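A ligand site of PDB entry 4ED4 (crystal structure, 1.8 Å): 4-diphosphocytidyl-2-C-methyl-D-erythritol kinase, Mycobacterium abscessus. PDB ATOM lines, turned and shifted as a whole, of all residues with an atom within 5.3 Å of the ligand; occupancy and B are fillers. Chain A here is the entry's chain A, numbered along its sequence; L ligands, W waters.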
ATOM      1  N   LYS A  25      -9.596 -18.028 -11.765  1.00  0.00           N
ATOM      2  CA  LYS A  25     -10.365 -18.584 -12.886  1.00  0.00           C
ATOM      3  C   LYS A  25     -11.846 -18.379 -12.779  1.00  0.00           C
ATOM      4  O   LYS A  25     -12.378 -18.118 -11.716  1.00  0.00           O
ATOM      5  CB  LYS A  25     -10.056 -20.085 -13.092  1.00  0.00           C
ATOM      6  CG  LYS A  25     -10.403 -21.029 -11.942  1.00  0.00           C
ATOM      7  CD  LYS A  25     -11.872 -21.420 -11.822  1.00  0.00           C
ATOM      8  CE  LYS A  25     -12.117 -22.395 -10.697  1.00  0.00           C
ATOM      9  NZ  LYS A  25     -13.583 -22.551 -10.382  1.00  0.00           N
ATOM     10  N   THR A  75      -7.676 -13.898   7.786  1.00  0.00           N
ATOM     11  CA  THR A  75      -8.295 -15.180   8.036  1.00  0.00           C
ATOM     12  C   THR A  75      -7.703 -16.389   7.326  1.00  0.00           C
ATOM     13  O   THR A  75      -7.870 -17.513   7.812  1.00  0.00           O
ATOM     14  CB  THR A  75      -9.743 -15.114   7.570  1.00  0.00           C
ATOM     15  OG1 THR A  75      -9.755 -14.444   6.296  1.00  0.00           O
ATOM     16  CG2 THR A  75     -10.568 -14.333   8.563  1.00  0.00           C
ATOM     17  N   VAL A  76      -7.039 -16.183   6.175  1.00  0.00           N
ATOM     18  CA  VAL A  76      -6.350 -17.265   5.490  1.00  0.00           C
ATOM     19  C   VAL A  76      -5.255 -17.836   6.396  1.00  0.00           C
ATOM     20  O   VAL A  76      -4.448 -17.094   6.928  1.00  0.00           O
ATOM     21  CB  VAL A  76      -5.764 -16.809   4.152  1.00  0.00           C
ATOM     22  CG1 VAL A  76      -4.813 -17.836   3.600  1.00  0.00           C
ATOM     23  CG2 VAL A  76      -6.929 -16.543   3.214  1.00  0.00           C
ATOM     24  N   PRO A  77      -5.303 -19.140   6.632  1.00  0.00           N
ATOM     25  CA  PRO A  77      -4.332 -19.713   7.537  1.00  0.00           C
ATOM     26  C   PRO A  77      -2.886 -19.643   7.035  1.00  0.00           C
ATOM     27  O   PRO A  77      -2.652 -19.659   5.835  1.00  0.00           O
ATOM     28  CB  PRO A  77      -4.763 -21.170   7.688  1.00  0.00           C
ATOM     29  CG  PRO A  77      -5.953 -21.381   6.828  1.00  0.00           C
ATOM     30  CD  PRO A  77      -6.174 -20.160   5.995  1.00  0.00           C
ATOM     31  N   ARG A  81      -2.458 -25.761   6.849  1.00  0.00           N
ATOM     32  CA  ARG A  81      -3.743 -25.690   6.138  1.00  0.00           C
ATOM     33  C   ARG A  81      -3.623 -24.994   4.810  1.00  0.00           C
ATOM     34  O   ARG A  81      -4.453 -25.210   3.931  1.00  0.00           O
ATOM     35  CB  ARG A  81      -4.788 -24.951   6.965  1.00  0.00           C
ATOM     36  CG  ARG A  81      -5.283 -25.747   8.198  1.00  0.00           C
ATOM     37  CD  ARG A  81      -6.137 -24.861   9.022  1.00  0.00           C
ATOM     38  NE  ARG A  81      -5.377 -23.894   9.801  1.00  0.00           N
ATOM     39  CZ  ARG A  81      -5.931 -23.011  10.592  1.00  0.00           C
ATOM     40  NH1 ARG A  81      -7.274 -22.895  10.685  1.00  0.00           N
ATOM     41  NH2 ARG A  81      -5.184 -22.228  11.309  1.00  0.00           N
ATOM     42  N   ASN A  82      -2.612 -24.136   4.668  1.00  0.00           N
ATOM     43  CA  ASN A  82      -2.507 -23.356   3.442  1.00  0.00           C
ATOM     44  C   ASN A  82      -2.005 -24.242   2.299  1.00  0.00           C
ATOM     45  O   ASN A  82      -1.018 -24.951   2.468  1.00  0.00           O
ATOM     46  CB  ASN A  82      -1.584 -22.173   3.680  1.00  0.00           C
ATOM     47  CG  ASN A  82      -1.736 -21.104   2.632  1.00  0.00           C
ATOM     48  OD1 ASN A  82      -1.451 -21.349   1.439  1.00  0.00           O
ATOM     49  ND2 ASN A  82      -2.157 -19.905   3.059  1.00  0.00           N
ATOM     50  N   LEU A  83      -2.659 -24.168   1.141  1.00  0.00           N
ATOM     51  CA  LEU A  83      -2.296 -24.990   0.032  1.00  0.00           C
ATOM     52  C   LEU A  83      -0.860 -24.620  -0.418  1.00  0.00           C
ATOM     53  O   LEU A  83      -0.111 -25.454  -0.949  1.00  0.00           O
ATOM     54  CB  LEU A  83      -3.318 -24.805  -1.102  1.00  0.00           C
ATOM     55  CG  LEU A  83      -3.400 -25.938  -2.113  1.00  0.00           C
ATOM     56  CD1 LEU A  83      -3.725 -27.308  -1.485  1.00  0.00           C
ATOM     57  CD2 LEU A  83      -4.445 -25.535  -3.175  1.00  0.00           C
ATOM     58  N   ALA A  84      -0.439 -23.391  -0.125  1.00  0.00           N
ATOM     59  CA  ALA A  84       0.925 -22.981  -0.518  1.00  0.00           C
ATOM     60  C   ALA A  84       1.969 -23.660   0.343  1.00  0.00           C
ATOM     61  O   ALA A  84       3.068 -23.914  -0.098  1.00  0.00           O
ATOM     62  CB  ALA A  84       1.085 -21.464  -0.448  1.00  0.00           C
ATOM     63  N   ILE A 105       2.003 -13.790   0.160  1.00  0.00           N
ATOM     64  CA  ILE A 105       0.906 -13.848  -0.795  1.00  0.00           C
ATOM     65  C   ILE A 105       0.124 -12.543  -0.723  1.00  0.00           C
ATOM     66  O   ILE A 105      -0.354 -12.170   0.316  1.00  0.00           O
ATOM     67  CB  ILE A 105      -0.057 -15.015  -0.500  1.00  0.00           C
ATOM     68  CG1 ILE A 105       0.733 -16.329  -0.286  1.00  0.00           C
ATOM     69  CG2 ILE A 105      -1.111 -15.100  -1.648  1.00  0.00           C
ATOM     70  CD1 ILE A 105      -0.105 -17.525   0.217  1.00  0.00           C
ATOM     71  N   LYS A 107      -3.055 -11.155  -2.174  1.00  0.00           N
ATOM     72  CA  LYS A 107      -4.225 -11.814  -2.781  1.00  0.00           C
ATOM     73  C   LYS A 107      -5.245 -10.803  -3.283  1.00  0.00           C
ATOM     74  O   LYS A 107      -5.742  -9.987  -2.521  1.00  0.00           O
ATOM     75  CB  LYS A 107      -4.953 -12.702  -1.762  1.00  0.00           C
ATOM     76  CG  LYS A 107      -4.234 -13.999  -1.389  1.00  0.00           C
ATOM     77  CD  LYS A 107      -5.046 -14.835  -0.398  1.00  0.00           C
ATOM     78  CE  LYS A 107      -6.213 -15.566  -1.041  1.00  0.00           C
ATOM     79  NZ  LYS A 107      -5.803 -16.454  -2.184  1.00  0.00           N
ATOM     80  N   PRO A 110     -10.758 -13.848  -4.460  1.00  0.00           N
ATOM     81  CA  PRO A 110     -11.542 -13.935  -3.216  1.00  0.00           C
ATOM     82  C   PRO A 110     -11.303 -15.246  -2.535  1.00  0.00           C
ATOM     83  O   PRO A 110     -11.101 -16.282  -3.215  1.00  0.00           O
ATOM     84  CB  PRO A 110     -12.990 -13.817  -3.698  1.00  0.00           C
ATOM     85  CG  PRO A 110     -12.934 -14.241  -5.101  1.00  0.00           C
ATOM     86  CD  PRO A 110     -11.612 -13.801  -5.648  1.00  0.00           C
ATOM     87  N   VAL A 111     -11.319 -15.252  -1.215  1.00  0.00           N
ATOM     88  CA  VAL A 111     -11.241 -16.489  -0.478  1.00  0.00           C
ATOM     89  C   VAL A 111     -12.578 -17.277  -0.548  1.00  0.00           C
ATOM     90  O   VAL A 111     -13.667 -16.741  -0.264  1.00  0.00           O
ATOM     91  CB  VAL A 111     -10.901 -16.199   1.018  1.00  0.00           C
ATOM     92  CG1 VAL A 111     -10.754 -17.490   1.832  1.00  0.00           C
ATOM     93  CG2 VAL A 111      -9.656 -15.357   1.096  1.00  0.00           C
ATOM     94  N   ALA A 112     -12.474 -18.572  -0.812  1.00  0.00           N
ATOM     95  CA  ALA A 112     -13.624 -19.512  -0.847  1.00  0.00           C
ATOM     96  C   ALA A 112     -14.703 -19.021  -1.791  1.00  0.00           C
ATOM     97  O   ALA A 112     -15.885 -19.155  -1.540  1.00  0.00           O
ATOM     98  CB  ALA A 112     -14.164 -19.794   0.576  1.00  0.00           C
ATOM     99  N   GLY A 113     -14.274 -18.436  -2.924  1.00  0.00           N
ATOM    100  CA  GLY A 113     -15.167 -17.759  -3.793  1.00  0.00           C
ATOM    101  C   GLY A 113     -15.411 -18.342  -5.140  1.00  0.00           C
ATOM    102  O   GLY A 113     -16.176 -17.784  -5.921  1.00  0.00           O
ATOM    103  N   GLY A 114     -14.850 -19.515  -5.399  1.00  0.00           N
ATOM    104  CA  GLY A 114     -15.049 -20.232  -6.655  1.00  0.00           C
ATOM    105  C   GLY A 114     -14.120 -19.808  -7.789  1.00  0.00           C
ATOM    106  O   GLY A 114     -14.373 -20.164  -8.941  1.00  0.00           O
ATOM    107  N   MET A 115     -13.082 -19.035  -7.477  1.00  0.00           N
ATOM    108  CA  MET A 115     -12.103 -18.633  -8.515  1.00  0.00           C
ATOM    109  C   MET A 115     -10.698 -19.288  -8.316  1.00  0.00           C
ATOM    110  O   MET A 115      -9.711 -18.903  -8.963  1.00  0.00           O
ATOM    111  CB  MET A 115     -11.980 -17.115  -8.546  1.00  0.00           C
ATOM    112  CG  MET A 115     -13.265 -16.376  -8.812  1.00  0.00           C
ATOM    113  SD  MET A 115     -13.102 -14.601  -9.063  1.00  0.00           S
ATOM    114  CE  MET A 115     -12.183 -14.505 -10.581  1.00  0.00           C
ATOM    115  N   ALA A 116     -10.639 -20.270  -7.425  1.00  0.00           N
ATOM    116  CA  ALA A 116      -9.468 -21.096  -7.169  1.00  0.00           C
ATOM    117  C   ALA A 116      -8.240 -20.245  -6.734  1.00  0.00           C
ATOM    118  O   ALA A 116      -7.177 -20.392  -7.266  1.00  0.00           O
ATOM    119  CB  ALA A 116      -9.132 -21.974  -8.384  1.00  0.00           C
ATOM    120  N   GLY A 117      -8.428 -19.363  -5.756  1.00  0.00           N
ATOM    121  CA  GLY A 117      -7.300 -18.566  -5.310  1.00  0.00           C
ATOM    122  C   GLY A 117      -6.217 -19.314  -4.553  1.00  0.00           C
ATOM    123  O   GLY A 117      -5.030 -19.009  -4.708  1.00  0.00           O
ATOM    124  N   GLY A 118      -6.582 -20.288  -3.718  1.00  0.00           N
ATOM    125  CA  GLY A 118      -5.575 -21.133  -3.042  1.00  0.00           C
ATOM    126  C   GLY A 118      -4.747 -21.948  -4.047  1.00  0.00           C
ATOM    127  O   GLY A 118      -3.527 -22.145  -3.871  1.00  0.00           O
ATOM    128  N   SER A 119      -5.420 -22.388  -5.122  1.00  0.00           N
ATOM    129  CA  SER A 119      -4.770 -23.066  -6.200  1.00  0.00           C
ATOM    130  C   SER A 119      -3.808 -22.192  -6.957  1.00  0.00           C
ATOM    131  O   SER A 119      -2.712 -22.650  -7.330  1.00  0.00           O
ATOM    132  CB  SER A 119      -5.823 -23.651  -7.129  1.00  0.00           C
ATOM    133  OG  SER A 119      -6.558 -24.640  -6.431  1.00  0.00           O
ATOM    134  N   ASP A 121      -2.182 -19.744  -5.605  1.00  0.00           N
ATOM    135  CA  ASP A 121      -1.099 -19.557  -4.652  1.00  0.00           C
ATOM    136  C   ASP A 121      -0.147 -20.742  -4.687  1.00  0.00           C
ATOM    137  O   ASP A 121       1.077 -20.572  -4.756  1.00  0.00           O
ATOM    138  CB  ASP A 121      -1.637 -19.333  -3.258  1.00  0.00           C
ATOM    139  CG  ASP A 121      -2.482 -18.035  -3.155  1.00  0.00           C
ATOM    140  OD1 ASP A 121      -2.453 -17.225  -4.124  1.00  0.00           O
ATOM    141  OD2 ASP A 121      -3.223 -17.910  -2.161  1.00  0.00           O
ATOM    142  N   ASP A 152      -7.739 -27.850  -9.083  1.00  0.00           N
ATOM    143  CA  ASP A 152      -7.649 -26.589  -9.814  1.00  0.00           C
ATOM    144  C   ASP A 152      -6.218 -26.028  -9.886  1.00  0.00           C
ATOM    145  O   ASP A 152      -5.982 -25.023 -10.517  1.00  0.00           O
ATOM    146  CB  ASP A 152      -8.593 -25.528  -9.163  1.00  0.00           C
ATOM    147  CG  ASP A 152     -10.073 -25.852  -9.379  1.00  0.00           C
ATOM    148  OD1 ASP A 152     -10.432 -26.549 -10.328  1.00  0.00           O
ATOM    149  OD2 ASP A 152     -10.916 -25.378  -8.625  1.00  0.00           O
ATOM    150  N   LEU A 191     -18.108 -20.156   0.199  1.00  0.00           N
ATOM    151  CA  LEU A 191     -18.648 -21.513   0.203  1.00  0.00           C
ATOM    152  C   LEU A 191     -17.523 -22.536   0.159  1.00  0.00           C
ATOM    153  O   LEU A 191     -16.534 -22.344  -0.536  1.00  0.00           O
ATOM    154  CB  LEU A 191     -19.553 -21.760  -0.988  1.00  0.00           C
ATOM    155  CG  LEU A 191     -20.960 -21.176  -0.868  1.00  0.00           C
ATOM    156  CD1 LEU A 191     -21.645 -21.118  -2.248  1.00  0.00           C
ATOM    157  CD2 LEU A 191     -21.744 -21.988   0.158  1.00  0.00           C
ATOM    158  N   THR A 193     -16.130 -25.770  -1.237  1.00  0.00           N
ATOM    159  CA  THR A 193     -16.426 -26.530  -2.463  1.00  0.00           C
ATOM    160  C   THR A 193     -16.991 -27.952  -2.183  1.00  0.00           C
ATOM    161  O   THR A 193     -17.922 -28.367  -2.849  1.00  0.00           O
ATOM    162  CB  THR A 193     -15.180 -26.578  -3.375  1.00  0.00           C
ATOM    163  OG1 THR A 193     -14.912 -25.263  -3.792  1.00  0.00           O
ATOM    164  CG2 THR A 193     -15.346 -27.506  -4.567  1.00  0.00           C
ATOM    165  N   SER A 269     -17.760 -23.224  -7.772  1.00  0.00           N
ATOM    166  CA  SER A 269     -18.637 -23.586  -6.664  1.00  0.00           C
ATOM    167  C   SER A 269     -19.193 -22.367  -5.916  1.00  0.00           C
ATOM    168  O   SER A 269     -19.937 -22.536  -4.973  1.00  0.00           O
ATOM    169  CB  SER A 269     -17.878 -24.445  -5.694  1.00  0.00           C
ATOM    170  OG  SER A 269     -16.649 -23.826  -5.288  1.00  0.00           O
ATOM    171  N   GLY A 270     -18.852 -21.158  -6.376  1.00  0.00           N
ATOM    172  CA  GLY A 270     -19.393 -19.909  -5.867  1.00  0.00           C
ATOM    173  C   GLY A 270     -18.723 -19.478  -4.552  1.00  0.00           C
ATOM    174  O   GLY A 270     -17.798 -20.109  -4.063  1.00  0.00           O
HETATM  175  P1  LIG L   1     -12.072 -23.809  -5.789  1.00  0.00           P
HETATM  176  O1  LIG L   1     -10.704 -24.245  -6.312  1.00  0.00           O
HETATM  177  O2  LIG L   1     -12.780 -22.802  -6.691  1.00  0.00           O
HETATM  178  O3  LIG L   1     -12.762 -25.036  -5.163  1.00  0.00           O
HETATM  179  P2  LIG L   1     -12.071 -21.533  -3.951  1.00  0.00           P
HETATM  180  O4  LIG L   1     -11.449 -20.363  -4.672  1.00  0.00           O
HETATM  181  O5  LIG L   1     -13.572 -21.576  -3.815  1.00  0.00           O
HETATM  182  O6  LIG L   1     -11.494 -22.872  -4.561  1.00  0.00           O
HETATM  183  P3  LIG L   1      -9.944 -21.055  -2.065  1.00  0.00           P
HETATM  184  O7  LIG L   1      -9.987 -19.560  -1.742  1.00  0.00           O
HETATM  185  O8  LIG L   1      -8.927 -21.569  -3.048  1.00  0.00           O
HETATM  186  O9  LIG L   1     -11.388 -21.569  -2.479  1.00  0.00           O
HETATM  187  O10 LIG L   1      -9.778 -21.987  -0.792  1.00  0.00           O
HETATM  188  C1  LIG L   1     -10.520 -21.674   0.418  1.00  0.00           C
HETATM  189  C2  LIG L   1     -10.288 -22.752   1.483  1.00  0.00           C
HETATM  190  O11 LIG L   1      -8.912 -23.183   1.526  1.00  0.00           O
HETATM  191  C3  LIG L   1     -10.574 -22.252   2.881  1.00  0.00           C
HETATM  192  O12 LIG L   1     -10.945 -23.419   3.664  1.00  0.00           O
HETATM  193  C4  LIG L   1      -9.237 -21.646   3.294  1.00  0.00           C
HETATM  194  O13 LIG L   1      -9.062 -21.496   4.743  1.00  0.00           O
HETATM  195  C5  LIG L   1      -8.282 -22.654   2.714  1.00  0.00           C
HETATM  196  N1  LIG L   1      -7.027 -22.117   2.179  1.00  0.00           N
HETATM  197  C6  LIG L   1      -5.859 -22.784   2.290  1.00  0.00           C
HETATM  198  N2  LIG L   1      -4.897 -22.092   1.640  1.00  0.00           N
HETATM  199  C7  LIG L   1      -5.465 -20.964   1.133  1.00  0.00           C
HETATM  200  C8  LIG L   1      -4.951 -19.824   0.357  1.00  0.00           C
HETATM  201  N3  LIG L   1      -3.627 -19.817   0.014  1.00  0.00           N
HETATM  202  N4  LIG L   1      -5.849 -18.900  -0.085  1.00  0.00           N
HETATM  203  C9  LIG L   1      -7.143 -18.939   0.325  1.00  0.00           C
HETATM  204  N5  LIG L   1      -7.660 -19.968   1.077  1.00  0.00           N
HETATM  205  C10 LIG L   1      -6.858 -20.981   1.477  1.00  0.00           C
HETATM  206  O   HOH W   1      -8.398 -23.925   6.269  1.00  0.00           O
HETATM  207  O   HOH W   2      -7.279 -23.705  -0.799  1.00  0.00           O
HETATM  208  O   HOH W   3     -16.156 -22.020  -3.215  1.00  0.00           O
HETATM  209  O   HOH W   4      -8.471 -23.362  -4.902  1.00  0.00           O
HETATM  210  O   HOH W   5     -13.564 -24.905   4.055  1.00  0.00           O
HETATM  211  O   HOH W   6      -8.550 -17.386  -2.516  1.00  0.00           O
HETATM  212  O   HOH W   7     -14.802 -23.784  -8.126  1.00  0.00           O
HETATM  213  O   HOH W   8     -10.143 -19.330   5.593  1.00  0.00           O
HETATM  214  O   HOH W   9     -11.605 -25.745  -2.584  1.00  0.00           O
HETATM  215  O   HOH W  10     -10.291 -26.070   2.707  1.00  0.00           O
HETATM  216  O   HOH W  11     -11.957 -18.003  -4.910  1.00  0.00           O
HETATM  217  O   HOH W  12     -13.645 -23.121   1.323  1.00  0.00           O
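An oxygen (O3) of the ligand sits at hydrogen-bond distance from the side-chain hydroxyl of Thr 193 (2.6 Å). The side-chain carboxylate of Asp 152 lies close to an oxygen (O1) of the ligand (2.6 Å). O8 of the ligand is in hydrogen-bond range of N of Gly 118, at 2.8 Å. An oxygen (O7) of the ligand sits at hydrogen-bond distance from the backbone NH (N) of Ala 112 (2.8 Å). O4 of the ligand is in hydrogen-bond range of N of Ala 116, at 2.9 Å. The backbone NH of Gly 114 lies within hydrogen-bond range of an oxygen (O5) of the ligand (2.9 Å). The side-chain carboxylate (OD2) of Asp 121 is in hydrogen-bond range of a nitrogen (N3) of the ligand (2.9 Å). A nitrogen (N3) of the ligand sits at hydrogen-bond distance from the side-chain amide oxygen (OD1) of Asn 82, at 3.0 Å. The backbone NH (N) of Leu 83 is in hydrogen-bond range of a nitrogen (N2) of the ligand, at 3.1 Å. The side-chain amino group (NZ) of Lys 107 sits at hydrogen-bond distance from a nitrogen (N4) of the ligand (3.2 Å). N of Gly 113 sits at hydrogen-bond distance from O5 of the ligand (3.3 Å). O4 of the ligand is in hydrogen-bond range of N of Gly 117 (3.4 Å). The side-chain amino group of Lys 25 is in salt-bridge range of an oxygen (O2) of the ligand (3.8 Å).
Water W4 bridges an oxygen (O8) of the ligand and the side-chain hydroxyl of Ser 119. Water W7 lies within hydrogen-bond range of an oxygen (O2) of the ligand (2.7 Å), the side-chain amino group of Lys 25 (2.8 Å) and the backbone NH of Ser 269 (3.0 Å). Water W6 lies within hydrogen-bond range of O7 of the ligand (2.7 Å), O of Pro 110 (2.9 Å) and NZ of Lys 107 (2.9 Å).
Merely in contact with the ligand: Val 76, Pro 77, Arg 81, Pro 110, Val 111 and Met 115. Of the 26 residues printed, 19 come within 4 Å of the ligand. The nearest printed residue that does not touch the ligand is Ser 269 (4.1 Å).
The side-chain hydroxyl (OG1) of Thr 193 sits at hydrogen-bond distance from the side-chain hydroxyl (OG) of Ser 269 (2.7 Å). The backbone carbonyl oxygen of Ala 112 sits at hydrogen-bond distance from the backbone NH of Leu 191, at 3.0 Å. O of Gly 114 is in hydrogen-bond range of NZ of Lys 25, at 2.9 Å. N of Gly 114 lies within hydrogen-bond range of O of Gly 270, at 3.3 Å. OD2 of Asp 121 is in salt-bridge range of NZ of Lys 107 (3.0 Å). O of Pro 77 lies within hydrogen-bond range of ND2 of Asn 82, 2.8 Å away. The side-chain amide oxygen of Asn 82 lies within hydrogen-bond range of the backbone NH of Ala 84 (2.8 Å). The backbone carbonyl oxygen of Met 115 lies within hydrogen-bond range of the backbone NH of Lys 25, 2.9 Å away.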
